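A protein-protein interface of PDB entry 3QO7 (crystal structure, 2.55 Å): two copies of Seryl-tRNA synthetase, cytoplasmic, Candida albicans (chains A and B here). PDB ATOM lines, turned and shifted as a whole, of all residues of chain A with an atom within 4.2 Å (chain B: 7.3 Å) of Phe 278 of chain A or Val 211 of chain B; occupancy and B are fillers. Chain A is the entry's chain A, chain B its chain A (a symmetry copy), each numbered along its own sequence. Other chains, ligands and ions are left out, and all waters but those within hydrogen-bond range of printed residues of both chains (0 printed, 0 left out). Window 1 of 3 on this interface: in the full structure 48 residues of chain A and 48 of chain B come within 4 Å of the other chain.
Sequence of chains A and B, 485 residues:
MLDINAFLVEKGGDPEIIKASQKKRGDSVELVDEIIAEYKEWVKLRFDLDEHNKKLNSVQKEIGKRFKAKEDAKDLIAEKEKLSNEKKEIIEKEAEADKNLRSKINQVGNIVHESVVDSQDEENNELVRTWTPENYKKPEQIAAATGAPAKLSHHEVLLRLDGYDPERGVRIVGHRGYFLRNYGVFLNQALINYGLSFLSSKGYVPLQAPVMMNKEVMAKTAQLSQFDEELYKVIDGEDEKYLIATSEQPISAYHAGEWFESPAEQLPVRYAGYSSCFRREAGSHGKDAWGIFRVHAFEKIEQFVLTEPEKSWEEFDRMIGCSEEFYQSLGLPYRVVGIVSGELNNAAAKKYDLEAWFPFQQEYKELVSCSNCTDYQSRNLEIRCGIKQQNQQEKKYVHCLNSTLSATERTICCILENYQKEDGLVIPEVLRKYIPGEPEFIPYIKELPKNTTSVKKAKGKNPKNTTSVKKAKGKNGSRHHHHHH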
ATOM      1  N   VAL A 211      20.002 -25.827  25.044  1.00  0.00           N
ATOM      2  CA  VAL A 211      19.226 -24.647  24.662  1.00  0.00           C
ATOM      3  C   VAL A 211      18.989 -23.707  25.820  1.00  0.00           C
ATOM      4  O   VAL A 211      18.271 -22.724  25.667  1.00  0.00           O
ATOM      5  CB  VAL A 211      17.862 -24.989  23.993  1.00  0.00           C
ATOM      6  CG1 VAL A 211      18.069 -25.938  22.837  1.00  0.00           C
ATOM      7  CG2 VAL A 211      16.872 -25.552  25.005  1.00  0.00           C
ATOM      8  N   TYR A 232      13.993 -15.431  26.054  1.00  0.00           N
ATOM      9  CA  TYR A 232      13.134 -15.950  27.106  1.00  0.00           C
ATOM     10  C   TYR A 232      13.964 -16.209  28.358  1.00  0.00           C
ATOM     11  O   TYR A 232      15.029 -16.817  28.296  1.00  0.00           O
ATOM     12  CB  TYR A 232      12.441 -17.248  26.669  1.00  0.00           C
ATOM     13  CG  TYR A 232      11.368 -17.083  25.603  1.00  0.00           C
ATOM     14  CD1 TYR A 232      10.055 -16.760  25.949  1.00  0.00           C
ATOM     15  CD2 TYR A 232      11.670 -17.264  24.239  1.00  0.00           C
ATOM     16  CE1 TYR A 232       9.072 -16.621  24.982  1.00  0.00           C
ATOM     17  CE2 TYR A 232      10.699 -17.128  23.263  1.00  0.00           C
ATOM     18  CZ  TYR A 232       9.394 -16.813  23.636  1.00  0.00           C
ATOM     19  OH  TYR A 232       8.414 -16.667  22.665  1.00  0.00           O
ATOM     20  N   LEU A 243      16.748 -19.147  27.434  1.00  0.00           N
ATOM     21  CA  LEU A 243      16.710 -20.006  26.279  1.00  0.00           C
ATOM     22  C   LEU A 243      17.529 -19.287  25.198  1.00  0.00           C
ATOM     23  O   LEU A 243      17.460 -18.049  25.054  1.00  0.00           O
ATOM     24  CB  LEU A 243      15.274 -20.259  25.848  1.00  0.00           C
ATOM     25  CG  LEU A 243      14.473 -21.136  26.812  1.00  0.00           C
ATOM     26  CD1 LEU A 243      13.006 -21.137  26.451  1.00  0.00           C
ATOM     27  CD2 LEU A 243      15.041 -22.559  26.823  1.00  0.00           C
ATOM     28  N   ILE A 244      18.333 -20.052  24.470  1.00  0.00           N
ATOM     29  CA  ILE A 244      19.160 -19.474  23.421  1.00  0.00           C
ATOM     30  C   ILE A 244      18.316 -19.032  22.209  1.00  0.00           C
ATOM     31  O   ILE A 244      17.275 -19.625  21.898  1.00  0.00           O
ATOM     32  CB  ILE A 244      20.262 -20.451  22.951  1.00  0.00           C
ATOM     33  CG1 ILE A 244      19.674 -21.581  22.122  1.00  0.00           C
ATOM     34  CG2 ILE A 244      21.055 -21.026  24.154  1.00  0.00           C
ATOM     35  CD1 ILE A 244      20.688 -22.674  21.812  1.00  0.00           C
ATOM     36  N   ALA A 245      18.772 -17.978  21.541  1.00  0.00           N
ATOM     37  CA  ALA A 245      18.190 -17.517  20.292  1.00  0.00           C
ATOM     38  C   ALA A 245      18.779 -18.241  19.084  1.00  0.00           C
ATOM     39  O   ALA A 245      18.217 -18.188  18.005  1.00  0.00           O
ATOM     40  CB  ALA A 245      18.424 -16.046  20.142  1.00  0.00           C
ATOM     41  N   SER A 276      17.395 -26.164  18.739  1.00  0.00           N
ATOM     42  CA  SER A 276      16.243 -25.283  18.604  1.00  0.00           C
ATOM     43  C   SER A 276      16.628 -23.869  19.072  1.00  0.00           C
ATOM     44  O   SER A 276      17.650 -23.677  19.732  1.00  0.00           O
ATOM     45  CB  SER A 276      15.032 -25.821  19.366  1.00  0.00           C
ATOM     46  OG  SER A 276      14.708 -27.108  18.876  1.00  0.00           O
ATOM     47  N   CYS A 277      15.811 -22.891  18.706  1.00  0.00           N
ATOM     48  CA  CYS A 277      16.124 -21.487  18.890  1.00  0.00           C
ATOM     49  C   CYS A 277      14.826 -20.869  19.310  1.00  0.00           C
ATOM     50  O   CYS A 277      13.772 -21.264  18.804  1.00  0.00           O
ATOM     51  CB  CYS A 277      16.569 -20.841  17.569  1.00  0.00           C
ATOM     52  SG  CYS A 277      17.971 -21.655  16.773  1.00  0.00           S
ATOM     53  N   PHE A 278      14.902 -19.901  20.220  1.00  0.00           N
ATOM     54  CA  PHE A 278      13.712 -19.319  20.822  1.00  0.00           C
ATOM     55  C   PHE A 278      13.806 -17.815  20.758  1.00  0.00           C
ATOM     56  O   PHE A 278      14.824 -17.217  21.145  1.00  0.00           O
ATOM     57  CB  PHE A 278      13.500 -19.842  22.254  1.00  0.00           C
ATOM     58  CG  PHE A 278      13.383 -21.342  22.317  1.00  0.00           C
ATOM     59  CD1 PHE A 278      12.141 -21.959  22.271  1.00  0.00           C
ATOM     60  CD2 PHE A 278      14.525 -22.142  22.343  1.00  0.00           C
ATOM     61  CE1 PHE A 278      12.036 -23.360  22.278  1.00  0.00           C
ATOM     62  CE2 PHE A 278      14.435 -23.519  22.336  1.00  0.00           C
ATOM     63  CZ  PHE A 278      13.180 -24.139  22.309  1.00  0.00           C
ATOM     64  N   ARG A 279      12.750 -17.202  20.232  1.00  0.00           N
ATOM     65  CA  ARG A 279      12.732 -15.757  20.079  1.00  0.00           C
ATOM     66  C   ARG A 279      11.445 -15.140  20.591  1.00  0.00           C
ATOM     67  O   ARG A 279      10.364 -15.490  20.122  1.00  0.00           O
ATOM     68  CB  ARG A 279      12.970 -15.404  18.622  1.00  0.00           C
ATOM     69  CG  ARG A 279      14.329 -15.860  18.132  1.00  0.00           C
ATOM     70  CD  ARG A 279      14.900 -14.916  17.087  1.00  0.00           C
ATOM     71  NE  ARG A 279      16.132 -15.452  16.521  1.00  0.00           N
ATOM     72  CZ  ARG A 279      16.676 -15.025  15.385  1.00  0.00           C
ATOM     73  NH1 ARG A 279      16.091 -14.045  14.692  1.00  0.00           N
ATOM     74  NH2 ARG A 279      17.804 -15.590  14.943  1.00  0.00           N
ATOM     75  N   HIS A 296       8.167 -18.335  17.138  1.00  0.00           N
ATOM     76  CA  HIS A 296       8.953 -18.173  18.393  1.00  0.00           C
ATOM     77  C   HIS A 296       9.960 -19.291  18.688  1.00  0.00           C
ATOM     78  O   HIS A 296      10.902 -19.097  19.458  1.00  0.00           O
ATOM     79  CB  HIS A 296       8.039 -18.022  19.596  1.00  0.00           C
ATOM     80  CG  HIS A 296       7.196 -16.794  19.552  1.00  0.00           C
ATOM     81  ND1 HIS A 296       7.714 -15.528  19.738  1.00  0.00           N
ATOM     82  CD2 HIS A 296       5.875 -16.632  19.320  1.00  0.00           C
ATOM     83  CE1 HIS A 296       6.744 -14.642  19.631  1.00  0.00           C
ATOM     84  NE2 HIS A 296       5.619 -15.284  19.383  1.00  0.00           N
ATOM     85  N   ALA A 297       9.750 -20.445  18.069  1.00  0.00           N
ATOM     86  CA  ALA A 297      10.618 -21.606  18.238  1.00  0.00           C
ATOM     87  C   ALA A 297      10.844 -22.294  16.886  1.00  0.00           C
ATOM     88  O   ALA A 297       9.914 -22.427  16.057  1.00  0.00           O
ATOM     89  CB  ALA A 297       9.998 -22.563  19.208  1.00  0.00           C
ATOM     90  N   GLN B 208       5.034 -33.144  15.653  1.00  0.00           N
ATOM     91  CA  GLN B 208       6.045 -32.432  16.432  1.00  0.00           C
ATOM     92  C   GLN B 208       5.376 -31.399  17.276  1.00  0.00           C
ATOM     93  O   GLN B 208       4.801 -30.454  16.748  1.00  0.00           O
ATOM     94  CB  GLN B 208       7.087 -31.747  15.529  1.00  0.00           C
ATOM     95  CG  GLN B 208       8.219 -31.001  16.308  1.00  0.00           C
ATOM     96  CD  GLN B 208       9.441 -30.734  15.438  1.00  0.00           C
ATOM     97  OE1 GLN B 208       9.748 -31.493  14.493  1.00  0.00           O
ATOM     98  NE2 GLN B 208      10.142 -29.633  15.733  1.00  0.00           N
ATOM     99  N   ALA B 209       5.454 -31.573  18.589  1.00  0.00           N
ATOM    100  CA  ALA B 209       4.763 -30.701  19.543  1.00  0.00           C
ATOM    101  C   ALA B 209       5.567 -29.450  19.860  1.00  0.00           C
ATOM    102  O   ALA B 209       6.782 -29.456  19.749  1.00  0.00           O
ATOM    103  CB  ALA B 209       4.467 -31.481  20.829  1.00  0.00           C
ATOM    104  N   PRO B 210       4.895 -28.361  20.250  1.00  0.00           N
ATOM    105  CA  PRO B 210       5.693 -27.184  20.630  1.00  0.00           C
ATOM    106  C   PRO B 210       6.167 -27.420  22.047  1.00  0.00           C
ATOM    107  O   PRO B 210       5.562 -28.260  22.695  1.00  0.00           O
ATOM    108  CB  PRO B 210       4.681 -26.031  20.543  1.00  0.00           C
ATOM    109  CG  PRO B 210       3.366 -26.675  20.751  1.00  0.00           C
ATOM    110  CD  PRO B 210       3.449 -28.071  20.200  1.00  0.00           C
ATOM    111  N   VAL B 211       7.222 -26.764  22.523  1.00  0.00           N
ATOM    112  CA  VAL B 211       7.759 -27.152  23.828  1.00  0.00           C
ATOM    113  C   VAL B 211       7.412 -26.163  24.917  1.00  0.00           C
ATOM    114  O   VAL B 211       7.876 -26.311  26.042  1.00  0.00           O
ATOM    115  CB  VAL B 211       9.298 -27.388  23.824  1.00  0.00           C
ATOM    116  CG1 VAL B 211       9.675 -28.365  22.736  1.00  0.00           C
ATOM    117  CG2 VAL B 211      10.062 -26.077  23.683  1.00  0.00           C
ATOM    118  N   MET B 212       6.613 -25.150  24.580  1.00  0.00           N
ATOM    119  CA  MET B 212       6.023 -24.287  25.592  1.00  0.00           C
ATOM    120  C   MET B 212       4.509 -24.462  25.632  1.00  0.00           C
ATOM    121  O   MET B 212       3.877 -24.704  24.605  1.00  0.00           O
ATOM    122  CB  MET B 212       6.358 -22.840  25.318  1.00  0.00           C
ATOM    123  CG  MET B 212       7.837 -22.511  25.364  1.00  0.00           C
ATOM    124  SD  MET B 212       8.103 -20.765  24.977  1.00  0.00           S
ATOM    125  CE  MET B 212       9.869 -20.582  25.103  1.00  0.00           C
ATOM    126  N   MET B 213       3.935 -24.335  26.830  1.00  0.00           N
ATOM    127  CA  MET B 213       2.487 -24.422  27.017  1.00  0.00           C
ATOM    128  C   MET B 213       1.991 -23.292  27.874  1.00  0.00           C
ATOM    129  O   MET B 213       2.677 -22.888  28.819  1.00  0.00           O
ATOM    130  CB  MET B 213       2.087 -25.740  27.688  1.00  0.00           C
ATOM    131  CG  MET B 213       1.828 -26.839  26.700  1.00  0.00           C
ATOM    132  SD  MET B 213       1.160 -28.359  27.396  1.00  0.00           S
ATOM    133  CE  MET B 213      -0.582 -27.958  27.568  1.00  0.00           C
ATOM    134  N   MET B 218      -1.880 -26.341  30.557  1.00  0.00           N
ATOM    135  CA  MET B 218      -0.999 -27.300  31.216  1.00  0.00           C
ATOM    136  C   MET B 218      -1.729 -27.836  32.442  1.00  0.00           C
ATOM    137  O   MET B 218      -1.743 -29.038  32.699  1.00  0.00           O
ATOM    138  CB  MET B 218       0.332 -26.637  31.612  1.00  0.00           C
ATOM    139  CG  MET B 218       1.295 -27.568  32.315  1.00  0.00           C
ATOM    140  SD  MET B 218       1.882 -28.974  31.323  1.00  0.00           S
ATOM    141  CE  MET B 218       3.317 -28.199  30.577  1.00  0.00           C
ATOM    142  N   TYR B 232       9.917 -26.219  34.256  1.00  0.00           N
ATOM    143  CA  TYR B 232      10.536 -24.911  34.124  1.00  0.00           C
ATOM    144  C   TYR B 232       9.471 -23.878  33.774  1.00  0.00           C
ATOM    145  O   TYR B 232       8.654 -24.090  32.880  1.00  0.00           O
ATOM    146  CB  TYR B 232      11.624 -24.917  33.042  1.00  0.00           C
ATOM    147  CG  TYR B 232      12.883 -25.697  33.393  1.00  0.00           C
ATOM    148  CD1 TYR B 232      13.918 -25.101  34.116  1.00  0.00           C
ATOM    149  CD2 TYR B 232      13.042 -27.036  32.986  1.00  0.00           C
ATOM    150  CE1 TYR B 232      15.072 -25.803  34.427  1.00  0.00           C
ATOM    151  CE2 TYR B 232      14.188 -27.749  33.290  1.00  0.00           C
ATOM    152  CZ  TYR B 232      15.210 -27.129  34.006  1.00  0.00           C
ATOM    153  OH  TYR B 232      16.360 -27.836  34.323  1.00  0.00           O
ATOM    154  N   VAL B 234       8.751 -20.286  32.057  1.00  0.00           N
ATOM    155  CA  VAL B 234       9.373 -19.419  31.081  1.00  0.00           C
ATOM    156  C   VAL B 234       8.802 -18.003  31.236  1.00  0.00           C
ATOM    157  O   VAL B 234       7.589 -17.835  31.345  1.00  0.00           O
ATOM    158  CB  VAL B 234       9.114 -19.949  29.658  1.00  0.00           C
ATOM    159  CG1 VAL B 234       9.429 -18.892  28.624  1.00  0.00           C
ATOM    160  CG2 VAL B 234       9.934 -21.207  29.394  1.00  0.00           C
ATOM    161  N   LYS B 241       4.761 -19.170  30.714  1.00  0.00           N
ATOM    162  CA  LYS B 241       4.417 -20.457  30.142  1.00  0.00           C
ATOM    163  C   LYS B 241       5.270 -21.483  30.851  1.00  0.00           C
ATOM    164  O   LYS B 241       6.086 -21.146  31.714  1.00  0.00           O
ATOM    165  CB  LYS B 241       4.721 -20.483  28.648  1.00  0.00           C
ATOM    166  CG  LYS B 241       4.122 -19.354  27.858  1.00  0.00           C
ATOM    167  CD  LYS B 241       4.548 -19.424  26.401  1.00  0.00           C
ATOM    168  CE  LYS B 241       3.992 -18.244  25.600  1.00  0.00           C
ATOM    169  NZ  LYS B 241       2.501 -18.142  25.601  1.00  0.00           N
ATOM    170  N   TYR B 242       5.086 -22.736  30.484  1.00  0.00           N
ATOM    171  CA  TYR B 242       5.941 -23.793  30.973  1.00  0.00           C
ATOM    172  C   TYR B 242       6.687 -24.409  29.812  1.00  0.00           C
ATOM    173  O   TYR B 242       6.200 -24.402  28.680  1.00  0.00           O
ATOM    174  CB  TYR B 242       5.113 -24.849  31.704  1.00  0.00           C
ATOM    175  CG  TYR B 242       4.522 -24.295  32.970  1.00  0.00           C
ATOM    176  CD1 TYR B 242       5.289 -24.172  34.119  1.00  0.00           C
ATOM    177  CD2 TYR B 242       3.214 -23.855  33.008  1.00  0.00           C
ATOM    178  CE1 TYR B 242       4.766 -23.646  35.275  1.00  0.00           C
ATOM    179  CE2 TYR B 242       2.677 -23.325  34.161  1.00  0.00           C
ATOM    180  CZ  TYR B 242       3.456 -23.219  35.293  1.00  0.00           C
ATOM    181  OH  TYR B 242       2.912 -22.686  36.441  1.00  0.00           O
ATOM    182  N   LEU B 243       7.890 -24.908  30.075  1.00  0.00           N
ATOM    183  CA  LEU B 243       8.471 -25.840  29.144  1.00  0.00           C
ATOM    184  C   LEU B 243       7.847 -27.202  29.475  1.00  0.00           C
ATOM    185  O   LEU B 243       7.646 -27.550  30.658  1.00  0.00           O
ATOM    186  CB  LEU B 243       9.987 -25.848  29.271  1.00  0.00           C
ATOM    187  CG  LEU B 243      10.665 -24.572  28.772  1.00  0.00           C
ATOM    188  CD1 LEU B 243      12.128 -24.552  29.155  1.00  0.00           C
ATOM    189  CD2 LEU B 243      10.490 -24.442  27.255  1.00  0.00           C
ATOM    190  N   ILE B 244       7.502 -27.955  28.438  1.00  0.00           N
ATOM    191  CA  ILE B 244       6.897 -29.263  28.634  1.00  0.00           C
ATOM    192  C   ILE B 244       7.918 -30.288  29.167  1.00  0.00           C
ATOM    193  O   ILE B 244       9.117 -30.218  28.870  1.00  0.00           O
ATOM    194  CB  ILE B 244       6.254 -29.804  27.337  1.00  0.00           C
ATOM    195  CG1 ILE B 244       7.318 -30.240  26.342  1.00  0.00           C
ATOM    196  CG2 ILE B 244       5.317 -28.751  26.691  1.00  0.00           C
ATOM    197  CD1 ILE B 244       6.740 -30.586  24.976  1.00  0.00           C
ATOM    198  N   ALA B 245       7.428 -31.229  29.967  1.00  0.00           N
ATOM    199  CA  ALA B 245       8.212 -32.359  30.438  1.00  0.00           C
ATOM    200  C   ALA B 245       8.195 -33.521  29.449  1.00  0.00           C
ATOM    201  O   ALA B 245       9.012 -34.418  29.544  1.00  0.00           O
ATOM    202  CB  ALA B 245       7.674 -32.828  31.755  1.00  0.00           C
ATOM    203  N   PRO B 250       1.465 -31.513  25.602  1.00  0.00           N
ATOM    204  CA  PRO B 250       0.769 -30.729  24.573  1.00  0.00           C
ATOM    205  C   PRO B 250      -0.100 -31.598  23.634  1.00  0.00           C
ATOM    206  O   PRO B 250      -1.137 -31.129  23.145  1.00  0.00           O
ATOM    207  CB  PRO B 250       1.914 -30.047  23.804  1.00  0.00           C
ATOM    208  CG  PRO B 250       3.161 -30.853  24.125  1.00  0.00           C
ATOM    209  CD  PRO B 250       2.940 -31.401  25.510  1.00  0.00           C
ATOM    210  N   TYR B 274       6.920 -36.196  18.799  1.00  0.00           N
ATOM    211  CA  TYR B 274       8.342 -35.921  18.913  1.00  0.00           C
ATOM    212  C   TYR B 274       8.528 -34.538  19.479  1.00  0.00           C
ATOM    213  O   TYR B 274       7.937 -33.585  18.958  1.00  0.00           O
ATOM    214  CB  TYR B 274       9.079 -35.983  17.553  1.00  0.00           C
ATOM    215  CG  TYR B 274      10.418 -35.275  17.633  1.00  0.00           C
ATOM    216  CD1 TYR B 274      11.388 -35.690  18.561  1.00  0.00           C
ATOM    217  CD2 TYR B 274      10.701 -34.171  16.844  1.00  0.00           C
ATOM    218  CE1 TYR B 274      12.624 -35.042  18.681  1.00  0.00           C
ATOM    219  CE2 TYR B 274      11.944 -33.494  16.957  1.00  0.00           C
ATOM    220  CZ  TYR B 274      12.899 -33.943  17.876  1.00  0.00           C
ATOM    221  OH  TYR B 274      14.124 -33.304  17.996  1.00  0.00           O
ATOM    222  N   SER B 275       9.353 -34.412  20.514  1.00  0.00           N
ATOM    223  CA  SER B 275       9.742 -33.086  20.986  1.00  0.00           C
ATOM    224  C   SER B 275      10.964 -33.188  21.876  1.00  0.00           C
ATOM    225  O   SER B 275      11.382 -34.286  22.191  1.00  0.00           O
ATOM    226  CB  SER B 275       8.616 -32.455  21.785  1.00  0.00           C
ATOM    227  OG  SER B 275       8.540 -33.032  23.065  1.00  0.00           O
ATOM    228  N   SER B 276      11.536 -32.055  22.273  1.00  0.00           N
ATOM    229  CA  SER B 276      12.422 -32.060  23.429  1.00  0.00           C
ATOM    230  C   SER B 276      11.580 -31.970  24.713  1.00  0.00           C
ATOM    231  O   SER B 276      10.398 -31.629  24.673  1.00  0.00           O
ATOM    232  CB  SER B 276      13.455 -30.937  23.348  1.00  0.00           C
ATOM    233  OG  SER B 276      14.215 -31.088  22.164  1.00  0.00           O
ATOM    234  N   CYS B 277      12.200 -32.295  25.839  1.00  0.00           N
ATOM    235  CA  CYS B 277      11.509 -32.454  27.105  1.00  0.00           C
ATOM    236  C   CYS B 277      12.437 -31.847  28.112  1.00  0.00           C
ATOM    237  O   CYS B 277      13.655 -31.995  27.986  1.00  0.00           O
ATOM    238  CB  CYS B 277      11.320 -33.939  27.449  1.00  0.00           C
ATOM    239  SG  CYS B 277      10.453 -34.894  26.184  1.00  0.00           S
ATOM    240  N   PHE B 278      11.864 -31.176  29.110  1.00  0.00           N
ATOM    241  CA  PHE B 278      12.648 -30.416  30.072  1.00  0.00           C
ATOM    242  C   PHE B 278      12.207 -30.776  31.469  1.00  0.00           C
ATOM    243  O   PHE B 278      11.005 -30.769  31.786  1.00  0.00           O
ATOM    244  CB  PHE B 278      12.560 -28.905  29.791  1.00  0.00           C
ATOM    245  CG  PHE B 278      13.022 -28.541  28.404  1.00  0.00           C
ATOM    246  CD1 PHE B 278      14.336 -28.165  28.170  1.00  0.00           C
ATOM    247  CD2 PHE B 278      12.155 -28.653  27.316  1.00  0.00           C
ATOM    248  CE1 PHE B 278      14.778 -27.875  26.869  1.00  0.00           C
ATOM    249  CE2 PHE B 278      12.582 -28.385  26.031  1.00  0.00           C
ATOM    250  CZ  PHE B 278      13.904 -27.986  25.801  1.00  0.00           C
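Printed residues of chain B within 4 Å of Phe 278 of chain A: Val 211 and Met 212. Of chain A, only Phe 278 (3.6 Å) comes within 4 Å of Val 211 of chain B. Of the printed residues of chain A, Phe 278 of chain B touches Val 211. Printed residues of chain A within 4 Å of Met 212 of chain B: Tyr 232 (3.8 Å), Leu 243 (3.5 Å) and Phe 278 (3.9 Å). Printed residues of chain B within 4 Å of Leu 243 of chain A: Met 212. Of the printed residues of chain B, Val 211 of chain A touches Phe 278. Ile 244 of chain A touches none of the printed residues of chain B. The nearest residue of chain B that does not touch Phe 278 of chain A is Phe 278 of chain B (5.2 Å). The nearest printed residue of chain A that does not touch Val 211 of chain B is Ala 297 of chain A (5.7 Å). The nearest printed residue of chain A that does not touch Val 234 of chain B is Leu 243 of chain A (4.3 Å).
Among the printed residues, merely in contact across the chains: Leu 243 of chain A with Met 212 of chain B, Tyr 232 of chain A with Val 234 of chain B, Phe 278 of chain A with Val 211 of chain B, Val 211 of chain A with Phe 278 of chain B, Tyr 232 of chain A with Met 212 of chain B and Phe 278 of chain A with Met 212 of chain B.
Val 211 of chain A touches Phe 278 of chain B, and with the chains exchanged Phe 278 of chain A touches Val 211 of chain B. Positions printed for both chains: 211, 232, 243, 244, 245, 276, 277 and 278. Of the 6 pairs that touch across the chains among the printed residues, 2 have their exchanged pair printed and touching as well.
OH of Tyr 232 of chain A sits at hydrogen-bond distance from ND1 of His 296 of chain A, at 3.2 Å. The backbone NH (N) of Val 234 of chain B sits at hydrogen-bond distance from the backbone carbonyl oxygen (O) of Lys 241 of chain B. O of Val 211 of chain B sits at hydrogen-bond distance from N of Ile 244 of chain B, 2.9 Å away. The backbone NH of Phe 278 of chain A is in hydrogen-bond range of the backbone carbonyl oxygen of Ile 244 of chain A, 2.9 Å away. The backbone carbonyl oxygen (O) of Arg 279 of chain A sits at hydrogen-bond distance from the side-chain hydroxyl (OH) of Tyr 232 of chain A (3.4 Å). The backbone NH (N) of Phe 278 of chain B lies within hydrogen-bond range of the backbone carbonyl oxygen (O) of Ile 244 of chain B (2.9 Å).
Hydrophobic or aromatic side chains of chain A that line the printed part of chain B: Val 211, Tyr 232, Leu 243 and Phe 278. Among the printed residues, 6 pairs touch across the chains. Among the printed residues, no Asp or Glu carboxylate lies within 4 Å of a Lys or Arg side-chain nitrogen of the other chain.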
